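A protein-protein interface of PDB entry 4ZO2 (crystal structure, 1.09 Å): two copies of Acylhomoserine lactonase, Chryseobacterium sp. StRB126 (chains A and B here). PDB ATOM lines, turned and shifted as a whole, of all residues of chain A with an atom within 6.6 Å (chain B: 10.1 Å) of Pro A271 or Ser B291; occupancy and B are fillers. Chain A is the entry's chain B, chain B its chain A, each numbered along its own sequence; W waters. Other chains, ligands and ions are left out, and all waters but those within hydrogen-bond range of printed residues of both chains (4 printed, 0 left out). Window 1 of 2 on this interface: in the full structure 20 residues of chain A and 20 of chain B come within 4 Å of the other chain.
Water W1 bridges the backbone carbonyl oxygen (O) of Pro B289 (2.7 Å) and the guanidinium group (NH2) of Arg A50 (3.2 Å).
Water W3 lies within hydrogen-bond range of O of Asn A48, NE of Arg A50 and O of Pro B289.
Water W4 lies within hydrogen-bond range of the backbone carbonyl oxygen of Met B293 (2.8 Å) and the side-chain amide oxygen of Asn A60 (2.8 Å).
Water W2 lies within hydrogen-bond range of the backbone carbonyl oxygen of Trp A272 (2.8 Å) and the backbone NH of Phe B292 (2.9 Å).
The side-chain hydroxyl (OG) of Ser B291 sits at hydrogen-bond distance from the guanidinium group (NE) of Arg A50 (3.4 Å).
The backbone NH (N) of Trp A272 lies within hydrogen-bond range of the backbone carbonyl oxygen (O) of Phe B292 (2.9 Å).
SD of Met B293 sits at hydrogen-bond distance from N of Ala A58, at 3.4 Å.
The guanidinium group (NH1) of Arg A50 lies within salt-bridge range of the side-chain carboxylate (OD1) of Asp A227, at 2.9 Å.
The backbone carbonyl oxygen (O) of Phe B277 is in hydrogen-bond range of the backbone NH (N) of Ile B288, at 2.8 Å.
The backbone carbonyl oxygen (O) of Ala A58 is in hydrogen-bond range of a ring nitrogen (ND1) of His A269, 2.7 Å away.
The chain-end carboxylate (O) of Asn B294 lies within salt-bridge range of the side-chain amino group (NZ) of Lys B7.
Positions printed for both chains: 272, 273, 274, 275, 287 and 289.
Ile B288 touches Asn A48.
Asp A56 touches Met B293.
Pro A271 touches Ser B291.
Phe B292 touches Pro A271.
Trp A272 touches Met B293.
N of Asn B294 touches CB of Trp A272 (3.5 Å).
Printed residues of chain B within 4 Å of Pro A271: Ser B291 and Phe B292.
Printed residues of chain A within 4 Å of Ser B291: Arg A50 (3.4 Å) and Pro A271 (3.9 Å).
No residue of chain B comes within 4 Å of Gly A274.
Of the printed residues of chain B, Arg A50 touches Ser B291 (3.4 Å).
Printed residues of chain B within 4 Å of Ala A58: Met B293 (3.4 Å).
Printed residues of chain A within 4 Å of Asn B294: Trp A272 (3.5 Å).
The nearest printed residue of chain B that does not touch Pro A271 is Met B293 (4.4 Å).
The nearest printed residue of chain A that does not touch Ser B291 is Asp A227 (5.6 Å).
Printed residues of chain B that touch a printed residue of chain A: Ile B288, Ser B291, Phe B292, Met B293 and Asn B294.
Hydrophobic or aromatic side chains of chain B within 4 Å of the printed part of chain A: Ile B288 and Met B293.
Hydrophobic or aromatic side chains of chain A that line the printed part of chain B: Ala A58, Pro A271 and Trp A272.
Among the printed residues, 9 pairs touch across the chains.
Among the printed residues, no Asp or Glu carboxylate lies within 4 Å of a Lys or Arg side-chain nitrogen of the other chain.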
ATOM      1  N   ASN A  48     -17.954  -7.392 -29.865  1.00  0.00           N
ATOM      2  CA  ASN A  48     -17.163  -6.634 -28.910  1.00  0.00           C
ATOM      3  C   ASN A  48     -15.933  -7.386 -28.413  1.00  0.00           C
ATOM      4  O   ASN A  48     -15.292  -6.951 -27.451  1.00  0.00           O
ATOM      5  CB  ASN A  48     -18.051  -6.196 -27.743  1.00  0.00           C
ATOM      6  CG  ASN A  48     -18.992  -5.093 -28.128  1.00  0.00           C
ATOM      7  OD1 ASN A  48     -18.599  -3.923 -28.104  1.00  0.00           O
ATOM      8  ND2 ASN A  48     -20.198  -5.435 -28.563  1.00  0.00           N
ATOM      9  N   ARG A  50     -15.492 -10.171 -26.986  1.00  0.00           N
ATOM     10  CA  ARG A  50     -15.645 -10.857 -25.729  1.00  0.00           C
ATOM     11  C   ARG A  50     -15.988 -12.321 -25.951  1.00  0.00           C
ATOM     12  O   ARG A  50     -16.475 -12.703 -27.003  1.00  0.00           O
ATOM     13  CB  ARG A  50     -16.741 -10.194 -24.895  1.00  0.00           C
ATOM     14  CG  ARG A  50     -16.468  -8.738 -24.677  1.00  0.00           C
ATOM     15  CD  ARG A  50     -17.389  -8.100 -23.691  1.00  0.00           C
ATOM     16  NE  ARG A  50     -17.185  -6.651 -23.631  1.00  0.00           N
ATOM     17  CZ  ARG A  50     -17.972  -5.823 -22.951  1.00  0.00           C
ATOM     18  NH1 ARG A  50     -19.006  -6.302 -22.282  1.00  0.00           N
ATOM     19  NH2 ARG A  50     -17.733  -4.515 -22.982  1.00  0.00           N
ATOM     20  N   ASP A  56     -18.815 -11.997 -17.665  1.00  0.00           N
ATOM     21  CA  ASP A  56     -18.266 -11.571 -16.386  1.00  0.00           C
ATOM     22  C   ASP A  56     -18.926 -10.274 -15.960  1.00  0.00           C
ATOM     23  O   ASP A  56     -18.892  -9.290 -16.712  1.00  0.00           O
ATOM     24  CB  ASP A  56     -16.749 -11.391 -16.478  1.00  0.00           C
ATOM     25  CG  ASP A  56     -16.004 -12.716 -16.472  1.00  0.00           C
ATOM     26  OD1 ASP A  56     -16.563 -13.734 -16.005  1.00  0.00           O
ATOM     27  OD2 ASP A  56     -14.846 -12.714 -16.922  1.00  0.00           O
ATOM     28  N   ALA A  58     -18.849  -7.335 -13.108  1.00  0.00           N
ATOM     29  CA  ALA A  58     -18.047  -6.738 -12.072  1.00  0.00           C
ATOM     30  C   ALA A  58     -18.873  -6.651 -10.783  1.00  0.00           C
ATOM     31  O   ALA A  58     -20.101  -6.739 -10.823  1.00  0.00           O
ATOM     32  CB  ALA A  58     -17.612  -5.344 -12.537  1.00  0.00           C
ATOM     33  N   ASN A  60     -18.641  -3.509  -8.478  1.00  0.00           N
ATOM     34  CA  ASN A  60     -18.077  -2.202  -8.184  1.00  0.00           C
ATOM     35  C   ASN A  60     -18.857  -1.583  -7.045  1.00  0.00           C
ATOM     36  O   ASN A  60     -20.088  -1.593  -7.071  1.00  0.00           O
ATOM     37  CB  ASN A  60     -18.152  -1.264  -9.408  1.00  0.00           C
ATOM     38  CG  ASN A  60     -17.672  -1.907 -10.684  1.00  0.00           C
ATOM     39  OD1 ASN A  60     -16.597  -2.515 -10.721  1.00  0.00           O
ATOM     40  ND2 ASN A  60     -18.467  -1.754 -11.760  1.00  0.00           N
ATOM     41  N   SER A 226     -25.634  -5.283 -18.267  1.00  0.00           N
ATOM     42  CA  SER A 226     -24.712  -5.462 -19.394  1.00  0.00           C
ATOM     43  C   SER A 226     -24.647  -4.189 -20.187  1.00  0.00           C
ATOM     44  O   SER A 226     -25.687  -3.669 -20.619  1.00  0.00           O
ATOM     45  CB  SER A 226     -25.161  -6.591 -20.343  1.00  0.00           C
ATOM     46  OG  SER A 226     -24.407  -6.587 -21.535  1.00  0.00           O
ATOM     47  N   ASP A 227     -23.427  -3.714 -20.428  1.00  0.00           N
ATOM     48  CA  ASP A 227     -23.204  -2.539 -21.259  1.00  0.00           C
ATOM     49  C   ASP A 227     -23.605  -2.805 -22.705  1.00  0.00           C
ATOM     50  O   ASP A 227     -24.324  -2.000 -23.309  1.00  0.00           O
ATOM     51  CB  ASP A 227     -21.751  -2.038 -21.143  1.00  0.00           C
ATOM     52  CG  ASP A 227     -20.668  -3.087 -21.417  1.00  0.00           C
ATOM     53  OD1 ASP A 227     -20.912  -4.310 -21.422  1.00  0.00           O
ATOM     54  OD2 ASP A 227     -19.518  -2.646 -21.652  1.00  0.00           O
ATOM     55  N   THR A 267     -22.234   2.211 -11.805  1.00  0.00           N
ATOM     56  CA  THR A 267     -22.993   0.982 -11.903  1.00  0.00           C
ATOM     57  C   THR A 267     -22.280  -0.128 -11.127  1.00  0.00           C
ATOM     58  O   THR A 267     -21.041  -0.202 -11.086  1.00  0.00           O
ATOM     59  CB  THR A 267     -23.144   0.551 -13.384  1.00  0.00           C
ATOM     60  OG1 THR A 267     -21.849   0.301 -13.943  1.00  0.00           O
ATOM     61  CG2 THR A 267     -23.870   1.591 -14.208  1.00  0.00           C
ATOM     62  N   HIS A 269     -22.320  -3.425 -11.885  1.00  0.00           N
ATOM     63  CA  HIS A 269     -21.934  -4.644 -12.575  1.00  0.00           C
ATOM     64  C   HIS A 269     -21.363  -4.447 -13.967  1.00  0.00           C
ATOM     65  O   HIS A 269     -20.920  -5.414 -14.563  1.00  0.00           O
ATOM     66  CB  HIS A 269     -23.129  -5.632 -12.633  1.00  0.00           C
ATOM     67  CG  HIS A 269     -23.618  -6.099 -11.288  1.00  0.00           C
ATOM     68  ND1 HIS A 269     -22.787  -6.672 -10.351  1.00  0.00           N
ATOM     69  CD2 HIS A 269     -24.854  -6.084 -10.718  1.00  0.00           C
ATOM     70  CE1 HIS A 269     -23.495  -7.003  -9.275  1.00  0.00           C
ATOM     71  NE2 HIS A 269     -24.758  -6.657  -9.465  1.00  0.00           N
ATOM     72  N   LEU A 270     -21.328  -3.217 -14.476  1.00  0.00           N
ATOM     73  CA  LEU A 270     -20.675  -2.975 -15.768  1.00  0.00           C
ATOM     74  C   LEU A 270     -19.142  -2.993 -15.597  1.00  0.00           C
ATOM     75  O   LEU A 270     -18.631  -2.912 -14.474  1.00  0.00           O
ATOM     76  CB  LEU A 270     -21.149  -1.656 -16.386  1.00  0.00           C
ATOM     77  CG  LEU A 270     -22.678  -1.477 -16.536  1.00  0.00           C
ATOM     78  CD1 LEU A 270     -22.901  -0.307 -17.476  1.00  0.00           C
ATOM     79  CD2 LEU A 270     -23.438  -2.699 -16.965  1.00  0.00           C
ATOM     80  N   PRO A 271     -18.395  -3.119 -16.702  1.00  0.00           N
ATOM     81  CA  PRO A 271     -16.940  -3.271 -16.553  1.00  0.00           C
ATOM     82  C   PRO A 271     -16.297  -2.121 -15.771  1.00  0.00           C
ATOM     83  O   PRO A 271     -16.749  -0.986 -15.786  1.00  0.00           O
ATOM     84  CB  PRO A 271     -16.444  -3.320 -17.991  1.00  0.00           C
ATOM     85  CG  PRO A 271     -17.615  -3.975 -18.735  1.00  0.00           C
ATOM     86  CD  PRO A 271     -18.825  -3.358 -18.098  1.00  0.00           C
ATOM     87  N   TRP A 272     -15.218  -2.470 -15.075  1.00  0.00           N
ATOM     88  CA  TRP A 272     -14.467  -1.566 -14.206  1.00  0.00           C
ATOM     89  C   TRP A 272     -14.022  -0.294 -14.933  1.00  0.00           C
ATOM     90  O   TRP A 272     -13.526  -0.386 -16.042  1.00  0.00           O
ATOM     91  CB  TRP A 272     -13.224  -2.293 -13.694  1.00  0.00           C
ATOM     92  CG  TRP A 272     -12.323  -1.455 -12.857  1.00  0.00           C
ATOM     93  CD1 TRP A 272     -11.192  -0.777 -13.258  1.00  0.00           C
ATOM     94  CD2 TRP A 272     -12.453  -1.217 -11.459  1.00  0.00           C
ATOM     95  NE1 TRP A 272     -10.637  -0.119 -12.192  1.00  0.00           N
ATOM     96  CE2 TRP A 272     -11.385  -0.382 -11.070  1.00  0.00           C
ATOM     97  CE3 TRP A 272     -13.381  -1.623 -10.491  1.00  0.00           C
ATOM     98  CZ2 TRP A 272     -11.211   0.041  -9.739  1.00  0.00           C
ATOM     99  CZ3 TRP A 272     -13.205  -1.216  -9.180  1.00  0.00           C
ATOM    100  CH2 TRP A 272     -12.130  -0.401  -8.813  1.00  0.00           C
ATOM    101  N   PRO A 273     -14.122   0.875 -14.297  1.00  0.00           N
ATOM    102  CA  PRO A 273     -14.591   1.130 -12.941  1.00  0.00           C
ATOM    103  C   PRO A 273     -16.092   1.474 -12.846  1.00  0.00           C
ATOM    104  O   PRO A 273     -16.516   2.051 -11.850  1.00  0.00           O
ATOM    105  CB  PRO A 273     -13.739   2.322 -12.510  1.00  0.00           C
ATOM    106  CG  PRO A 273     -13.624   3.116 -13.785  1.00  0.00           C
ATOM    107  CD  PRO A 273     -13.457   2.074 -14.858  1.00  0.00           C
ATOM    108  N   GLY A 274     -16.886   1.122 -13.857  1.00  0.00           N
ATOM    109  CA  GLY A 274     -18.330   1.174 -13.743  1.00  0.00           C
ATOM    110  C   GLY A 274     -18.930   2.540 -13.996  1.00  0.00           C
ATOM    111  O   GLY A 274     -20.126   2.739 -13.741  1.00  0.00           O
ATOM    112  N   LEU A 275     -18.111   3.484 -14.471  1.00  0.00           N
ATOM    113  CA  LEU A 275     -18.488   4.884 -14.663  1.00  0.00           C
ATOM    114  C   LEU A 275     -18.728   5.219 -16.139  1.00  0.00           C
ATOM    115  O   LEU A 275     -17.912   4.855 -16.992  1.00  0.00           O
ATOM    116  CB  LEU A 275     -17.376   5.794 -14.148  1.00  0.00           C
ATOM    117  CG  LEU A 275     -17.202   5.830 -12.636  1.00  0.00           C
ATOM    118  CD1 LEU A 275     -15.849   6.408 -12.235  1.00  0.00           C
ATOM    119  CD2 LEU A 275     -18.319   6.656 -11.975  1.00  0.00           C
ATOM    120  N   TRP A 287     -24.010   2.708 -23.918  1.00  0.00           N
ATOM    121  CA  TRP A 287     -23.131   3.076 -22.804  1.00  0.00           C
ATOM    122  C   TRP A 287     -21.804   3.572 -23.338  1.00  0.00           C
ATOM    123  O   TRP A 287     -21.168   2.884 -24.138  1.00  0.00           O
ATOM    124  CB  TRP A 287     -22.888   1.864 -21.929  1.00  0.00           C
ATOM    125  CG  TRP A 287     -21.949   2.042 -20.747  1.00  0.00           C
ATOM    126  CD1 TRP A 287     -20.734   1.423 -20.580  1.00  0.00           C
ATOM    127  CD2 TRP A 287     -22.207   2.746 -19.510  1.00  0.00           C
ATOM    128  NE1 TRP A 287     -20.229   1.709 -19.327  1.00  0.00           N
ATOM    129  CE2 TRP A 287     -21.114   2.505 -18.658  1.00  0.00           C
ATOM    130  CE3 TRP A 287     -23.245   3.570 -19.053  1.00  0.00           C
ATOM    131  CZ2 TRP A 287     -21.056   3.012 -17.348  1.00  0.00           C
ATOM    132  CZ3 TRP A 287     -23.198   4.061 -17.761  1.00  0.00           C
ATOM    133  CH2 TRP A 287     -22.110   3.790 -16.919  1.00  0.00           C
ATOM    134  N   PRO A 289     -18.308   4.410 -21.836  1.00  0.00           N
ATOM    135  CA  PRO A 289     -17.523   4.418 -20.601  1.00  0.00           C
ATOM    136  C   PRO A 289     -16.699   5.677 -20.468  1.00  0.00           C
ATOM    137  O   PRO A 289     -16.187   6.221 -21.450  1.00  0.00           O
ATOM    138  CB  PRO A 289     -16.626   3.177 -20.722  1.00  0.00           C
ATOM    139  CG  PRO A 289     -16.789   2.651 -22.086  1.00  0.00           C
ATOM    140  CD  PRO A 289     -17.900   3.357 -22.786  1.00  0.00           C
ATOM    141  N   LYS B   7      -0.975  -2.145 -14.010  1.00  0.00           N
ATOM    142  CA  LYS B   7      -1.909  -3.234 -14.136  1.00  0.00           C
ATOM    143  C   LYS B   7      -1.159  -4.477 -14.591  1.00  0.00           C
ATOM    144  O   LYS B   7      -0.487  -4.452 -15.609  1.00  0.00           O
ATOM    145  CB  LYS B   7      -3.006  -2.876 -15.127  1.00  0.00           C
ATOM    146  CG  LYS B   7      -3.982  -3.994 -15.329  1.00  0.00           C
ATOM    147  CD  LYS B   7      -5.060  -3.604 -16.307  1.00  0.00           C
ATOM    148  CE  LYS B   7      -6.186  -4.620 -16.387  1.00  0.00           C
ATOM    149  NZ  LYS B   7      -6.878  -4.842 -15.101  1.00  0.00           N
ATOM    150  N   ILE B   9      -1.193  -8.262 -16.181  1.00  0.00           N
ATOM    151  CA  ILE B   9      -1.943  -9.246 -16.927  1.00  0.00           C
ATOM    152  C   ILE B   9      -1.025 -10.400 -17.303  1.00  0.00           C
ATOM    153  O   ILE B   9       0.190 -10.300 -17.208  1.00  0.00           O
ATOM    154  CB  ILE B   9      -2.593  -8.651 -18.201  1.00  0.00           C
ATOM    155  CG1 ILE B   9      -1.525  -8.260 -19.204  1.00  0.00           C
ATOM    156  CG2 ILE B   9      -3.495  -7.471 -17.865  1.00  0.00           C
ATOM    157  CD1 ILE B   9      -2.058  -7.831 -20.615  1.00  0.00           C
ATOM    158  N   ARG B 264      -5.443  -8.305 -30.567  1.00  0.00           N
ATOM    159  CA  ARG B 264      -5.379  -7.295 -29.525  1.00  0.00           C
ATOM    160  C   ARG B 264      -4.122  -6.431 -29.713  1.00  0.00           C
ATOM    161  O   ARG B 264      -3.040  -6.947 -30.018  1.00  0.00           O
ATOM    162  CB  ARG B 264      -5.368  -7.945 -28.138  1.00  0.00           C
ATOM    163  CG  ARG B 264      -5.478  -6.917 -27.019  1.00  0.00           C
ATOM    164  CD  ARG B 264      -5.760  -7.556 -25.660  1.00  0.00           C
ATOM    165  NE  ARG B 264      -4.719  -8.525 -25.324  1.00  0.00           N
ATOM    166  CZ  ARG B 264      -4.405  -8.900 -24.082  1.00  0.00           C
ATOM    167  NH1 ARG B 264      -4.990  -8.326 -23.030  1.00  0.00           N
ATOM    168  NH2 ARG B 264      -3.466  -9.813 -23.886  1.00  0.00           N
ATOM    169  N   TRP B 272      -6.162   4.617 -20.662  1.00  0.00           N
ATOM    170  CA  TRP B 272      -5.700   3.537 -19.809  1.00  0.00           C
ATOM    171  C   TRP B 272      -6.658   2.341 -19.783  1.00  0.00           C
ATOM    172  O   TRP B 272      -7.853   2.557 -19.633  1.00  0.00           O
ATOM    173  CB  TRP B 272      -5.532   4.079 -18.390  1.00  0.00           C
ATOM    174  CG  TRP B 272      -5.110   3.040 -17.383  1.00  0.00           C
ATOM    175  CD1 TRP B 272      -5.918   2.328 -16.555  1.00  0.00           C
ATOM    176  CD2 TRP B 272      -3.775   2.606 -17.128  1.00  0.00           C
ATOM    177  NE1 TRP B 272      -5.157   1.471 -15.772  1.00  0.00           N
ATOM    178  CE2 TRP B 272      -3.836   1.642 -16.102  1.00  0.00           C
ATOM    179  CE3 TRP B 272      -2.526   2.968 -17.643  1.00  0.00           C
ATOM    180  CZ2 TRP B 272      -2.687   1.025 -15.591  1.00  0.00           C
ATOM    181  CZ3 TRP B 272      -1.389   2.358 -17.130  1.00  0.00           C
ATOM    182  CH2 TRP B 272      -1.477   1.409 -16.123  1.00  0.00           C
ATOM    183  N   PRO B 273      -6.148   1.096 -19.842  1.00  0.00           N
ATOM    184  CA  PRO B 273      -4.749   0.691 -19.900  1.00  0.00           C
ATOM    185  C   PRO B 273      -4.192   0.497 -21.324  1.00  0.00           C
ATOM    186  O   PRO B 273      -3.165  -0.151 -21.470  1.00  0.00           O
ATOM    187  CB  PRO B 273      -4.743  -0.643 -19.134  1.00  0.00           C
ATOM    188  CG  PRO B 273      -6.050  -1.257 -19.541  1.00  0.00           C
ATOM    189  CD  PRO B 273      -7.014  -0.074 -19.546  1.00  0.00           C
ATOM    190  N   GLY B 274      -4.853   1.066 -22.331  1.00  0.00           N
ATOM    191  CA  GLY B 274      -4.279   1.119 -23.653  1.00  0.00           C
ATOM    192  C   GLY B 274      -4.437  -0.150 -24.477  1.00  0.00           C
ATOM    193  O   GLY B 274      -3.839  -0.237 -25.553  1.00  0.00           O
ATOM    194  N   LEU B 275      -5.248  -1.102 -24.003  1.00  0.00           N
ATOM    195  CA  LEU B 275      -5.456  -2.414 -24.606  1.00  0.00           C
ATOM    196  C   LEU B 275      -6.781  -2.471 -25.324  1.00  0.00           C
ATOM    197  O   LEU B 275      -7.800  -2.061 -24.768  1.00  0.00           O
ATOM    198  CB  LEU B 275      -5.434  -3.490 -23.515  1.00  0.00           C
ATOM    199  CG  LEU B 275      -4.071  -3.743 -22.878  1.00  0.00           C
ATOM    200  CD1 LEU B 275      -4.282  -4.526 -21.586  1.00  0.00           C
ATOM    201  CD2 LEU B 275      -3.172  -4.493 -23.823  1.00  0.00           C
ATOM    202  N   GLY B 276      -6.811  -3.042 -26.514  1.00  0.00           N
ATOM    203  CA  GLY B 276      -8.073  -3.095 -27.219  1.00  0.00           C
ATOM    204  C   GLY B 276      -7.988  -3.684 -28.603  1.00  0.00           C
ATOM    205  O   GLY B 276      -6.943  -4.151 -29.062  1.00  0.00           O
ATOM    206  N   PHE B 277      -9.148  -3.673 -29.248  1.00  0.00           N
ATOM    207  CA  PHE B 277      -9.405  -4.361 -30.508  1.00  0.00           C
ATOM    208  C   PHE B 277      -9.853  -3.349 -31.545  1.00  0.00           C
ATOM    209  O   PHE B 277     -10.371  -2.283 -31.196  1.00  0.00           O
ATOM    210  CB  PHE B 277     -10.476  -5.440 -30.292  1.00  0.00           C
ATOM    211  CG  PHE B 277     -10.063  -6.456 -29.293  1.00  0.00           C
ATOM    212  CD1 PHE B 277      -9.370  -7.585 -29.689  1.00  0.00           C
ATOM    213  CD2 PHE B 277     -10.346  -6.280 -27.949  1.00  0.00           C
ATOM    214  CE1 PHE B 277      -8.970  -8.547 -28.756  1.00  0.00           C
ATOM    215  CE2 PHE B 277      -9.959  -7.230 -27.012  1.00  0.00           C
ATOM    216  CZ  PHE B 277      -9.271  -8.369 -27.425  1.00  0.00           C
ATOM    217  N   TRP B 287     -12.217   1.652 -32.319  1.00  0.00           N
ATOM    218  CA  TRP B 287     -11.497   1.024 -31.217  1.00  0.00           C
ATOM    219  C   TRP B 287     -12.478   0.477 -30.197  1.00  0.00           C
ATOM    220  O   TRP B 287     -13.354   1.207 -29.734  1.00  0.00           O
ATOM    221  CB  TRP B 287     -10.600   2.053 -30.542  1.00  0.00           C
ATOM    222  CG  TRP B 287      -9.785   1.632 -29.339  1.00  0.00           C
ATOM    223  CD1 TRP B 287      -9.931   2.097 -28.065  1.00  0.00           C
ATOM    224  CD2 TRP B 287      -8.629   0.762 -29.323  1.00  0.00           C
ATOM    225  NE1 TRP B 287      -8.929   1.577 -27.265  1.00  0.00           N
ATOM    226  CE2 TRP B 287      -8.114   0.777 -28.023  1.00  0.00           C
ATOM    227  CE3 TRP B 287      -7.959   0.020 -30.301  1.00  0.00           C
ATOM    228  CZ2 TRP B 287      -6.939   0.097 -27.675  1.00  0.00           C
ATOM    229  CZ3 TRP B 287      -6.802  -0.655 -29.968  1.00  0.00           C
ATOM    230  CH2 TRP B 287      -6.302  -0.622 -28.661  1.00  0.00           C
ATOM    231  N   ILE B 288     -12.303  -0.793 -29.844  1.00  0.00           N
ATOM    232  CA  ILE B 288     -13.105  -1.421 -28.802  1.00  0.00           C
ATOM    233  C   ILE B 288     -12.149  -1.693 -27.635  1.00  0.00           C
ATOM    234  O   ILE B 288     -11.311  -2.588 -27.709  1.00  0.00           O
ATOM    235  CB  ILE B 288     -13.761  -2.738 -29.254  1.00  0.00           C
ATOM    236  CG1 ILE B 288     -14.535  -2.563 -30.562  1.00  0.00           C
ATOM    237  CG2 ILE B 288     -14.673  -3.256 -28.113  1.00  0.00           C
ATOM    238  CD1 ILE B 288     -15.645  -1.606 -30.462  1.00  0.00           C
ATOM    239  N   PRO B 289     -12.225  -0.894 -26.553  1.00  0.00           N
ATOM    240  CA  PRO B 289     -11.287  -1.131 -25.461  1.00  0.00           C
ATOM    241  C   PRO B 289     -11.569  -2.482 -24.835  1.00  0.00           C
ATOM    242  O   PRO B 289     -12.709  -2.902 -24.705  1.00  0.00           O
ATOM    243  CB  PRO B 289     -11.545   0.044 -24.490  1.00  0.00           C
ATOM    244  CG  PRO B 289     -12.856   0.598 -24.885  1.00  0.00           C
ATOM    245  CD  PRO B 289     -13.154   0.216 -26.293  1.00  0.00           C
ATOM    246  N   GLU B 290     -10.514  -3.143 -24.387  1.00  0.00           N
ATOM    247  CA  GLU B 290     -10.689  -4.382 -23.637  1.00  0.00           C
ATOM    248  C   GLU B 290     -11.426  -4.067 -22.333  1.00  0.00           C
ATOM    249  O   GLU B 290     -11.202  -3.040 -21.719  1.00  0.00           O
ATOM    250  CB  GLU B 290      -9.329  -5.040 -23.358  1.00  0.00           C
ATOM    251  CG  GLU B 290      -9.485  -6.370 -22.655  1.00  0.00           C
ATOM    252  CD  GLU B 290      -8.170  -7.124 -22.492  1.00  0.00           C
ATOM    253  OE1 GLU B 290      -7.128  -6.621 -22.939  1.00  0.00           O
ATOM    254  OE2 GLU B 290      -8.176  -8.235 -21.897  1.00  0.00           O
ATOM    255  N   SER B 291     -12.326  -4.962 -21.952  1.00  0.00           N
ATOM    256  CA  SER B 291     -13.110  -4.791 -20.732  1.00  0.00           C
ATOM    257  C   SER B 291     -12.514  -5.618 -19.595  1.00  0.00           C
ATOM    258  O   SER B 291     -12.056  -6.759 -19.788  1.00  0.00           O
ATOM    259  CB  SER B 291     -14.593  -5.173 -20.946  1.00  0.00           C
ATOM    260  OG  SER B 291     -14.747  -6.543 -21.280  1.00  0.00           O
ATOM    261  N   PHE B 292     -12.495  -5.009 -18.422  1.00  0.00           N
ATOM    262  CA  PHE B 292     -11.879  -5.584 -17.232  1.00  0.00           C
ATOM    263  C   PHE B 292     -12.818  -5.552 -16.047  1.00  0.00           C
ATOM    264  O   PHE B 292     -13.742  -4.740 -15.996  1.00  0.00           O
ATOM    265  CB  PHE B 292     -10.591  -4.847 -16.876  1.00  0.00           C
ATOM    266  CG  PHE B 292      -9.546  -4.912 -17.958  1.00  0.00           C
ATOM    267  CD1 PHE B 292      -8.761  -6.038 -18.108  1.00  0.00           C
ATOM    268  CD2 PHE B 292      -9.374  -3.854 -18.836  1.00  0.00           C
ATOM    269  CE1 PHE B 292      -7.799  -6.108 -19.106  1.00  0.00           C
ATOM    270  CE2 PHE B 292      -8.416  -3.915 -19.841  1.00  0.00           C
ATOM    271  CZ  PHE B 292      -7.637  -5.040 -19.968  1.00  0.00           C
ATOM    272  N   MET B 293     -12.544  -6.439 -15.081  1.00  0.00           N
ATOM    273  CA  MET B 293     -13.293  -6.485 -13.838  1.00  0.00           C
ATOM    274  C   MET B 293     -12.626  -5.676 -12.726  1.00  0.00           C
ATOM    275  O   MET B 293     -13.223  -5.471 -11.678  1.00  0.00           O
ATOM    276  CB  MET B 293     -13.449  -7.942 -13.389  1.00  0.00           C
ATOM    277  CG  MET B 293     -14.264  -8.809 -14.337  1.00  0.00           C
ATOM    278  SD  MET B 293     -15.954  -8.332 -14.468  1.00  0.00           S
ATOM    279  CE  MET B 293     -16.036  -7.508 -16.071  1.00  0.00           C
ATOM    280  N   ASN B 294     -11.395  -5.226 -12.953  1.00  0.00           N
ATOM    281  CA  ASN B 294     -10.640  -4.493 -11.947  1.00  0.00           C
ATOM    282  C   ASN B 294      -9.469  -3.818 -12.630  1.00  0.00           C
ATOM    283  O   ASN B 294      -9.379  -3.914 -13.872  1.00  0.00           O
ATOM    284  CB  ASN B 294     -10.182  -5.422 -10.815  1.00  0.00           C
ATOM    285  CG  ASN B 294      -9.527  -6.664 -11.364  1.00  0.00           C
ATOM    286  OD1 ASN B 294      -8.564  -6.546 -12.105  1.00  0.00           O
ATOM    287  ND2 ASN B 294     -10.102  -7.831 -11.114  1.00  0.00           N
ATOM    288  OXT ASN B 294      -8.642  -3.207 -11.946  1.00  0.00           O
HETATM  289  O   HOH W   1     -15.397  -2.841 -24.347  1.00  0.00           O
HETATM  290  O   HOH W   2     -13.014  -2.179 -18.161  1.00  0.00           O
HETATM  291  O   HOH W   3     -14.786  -5.693 -25.076  1.00  0.00           O
HETATM  292  O   HOH W   4     -15.375  -4.947  -9.970  1.00  0.00           O
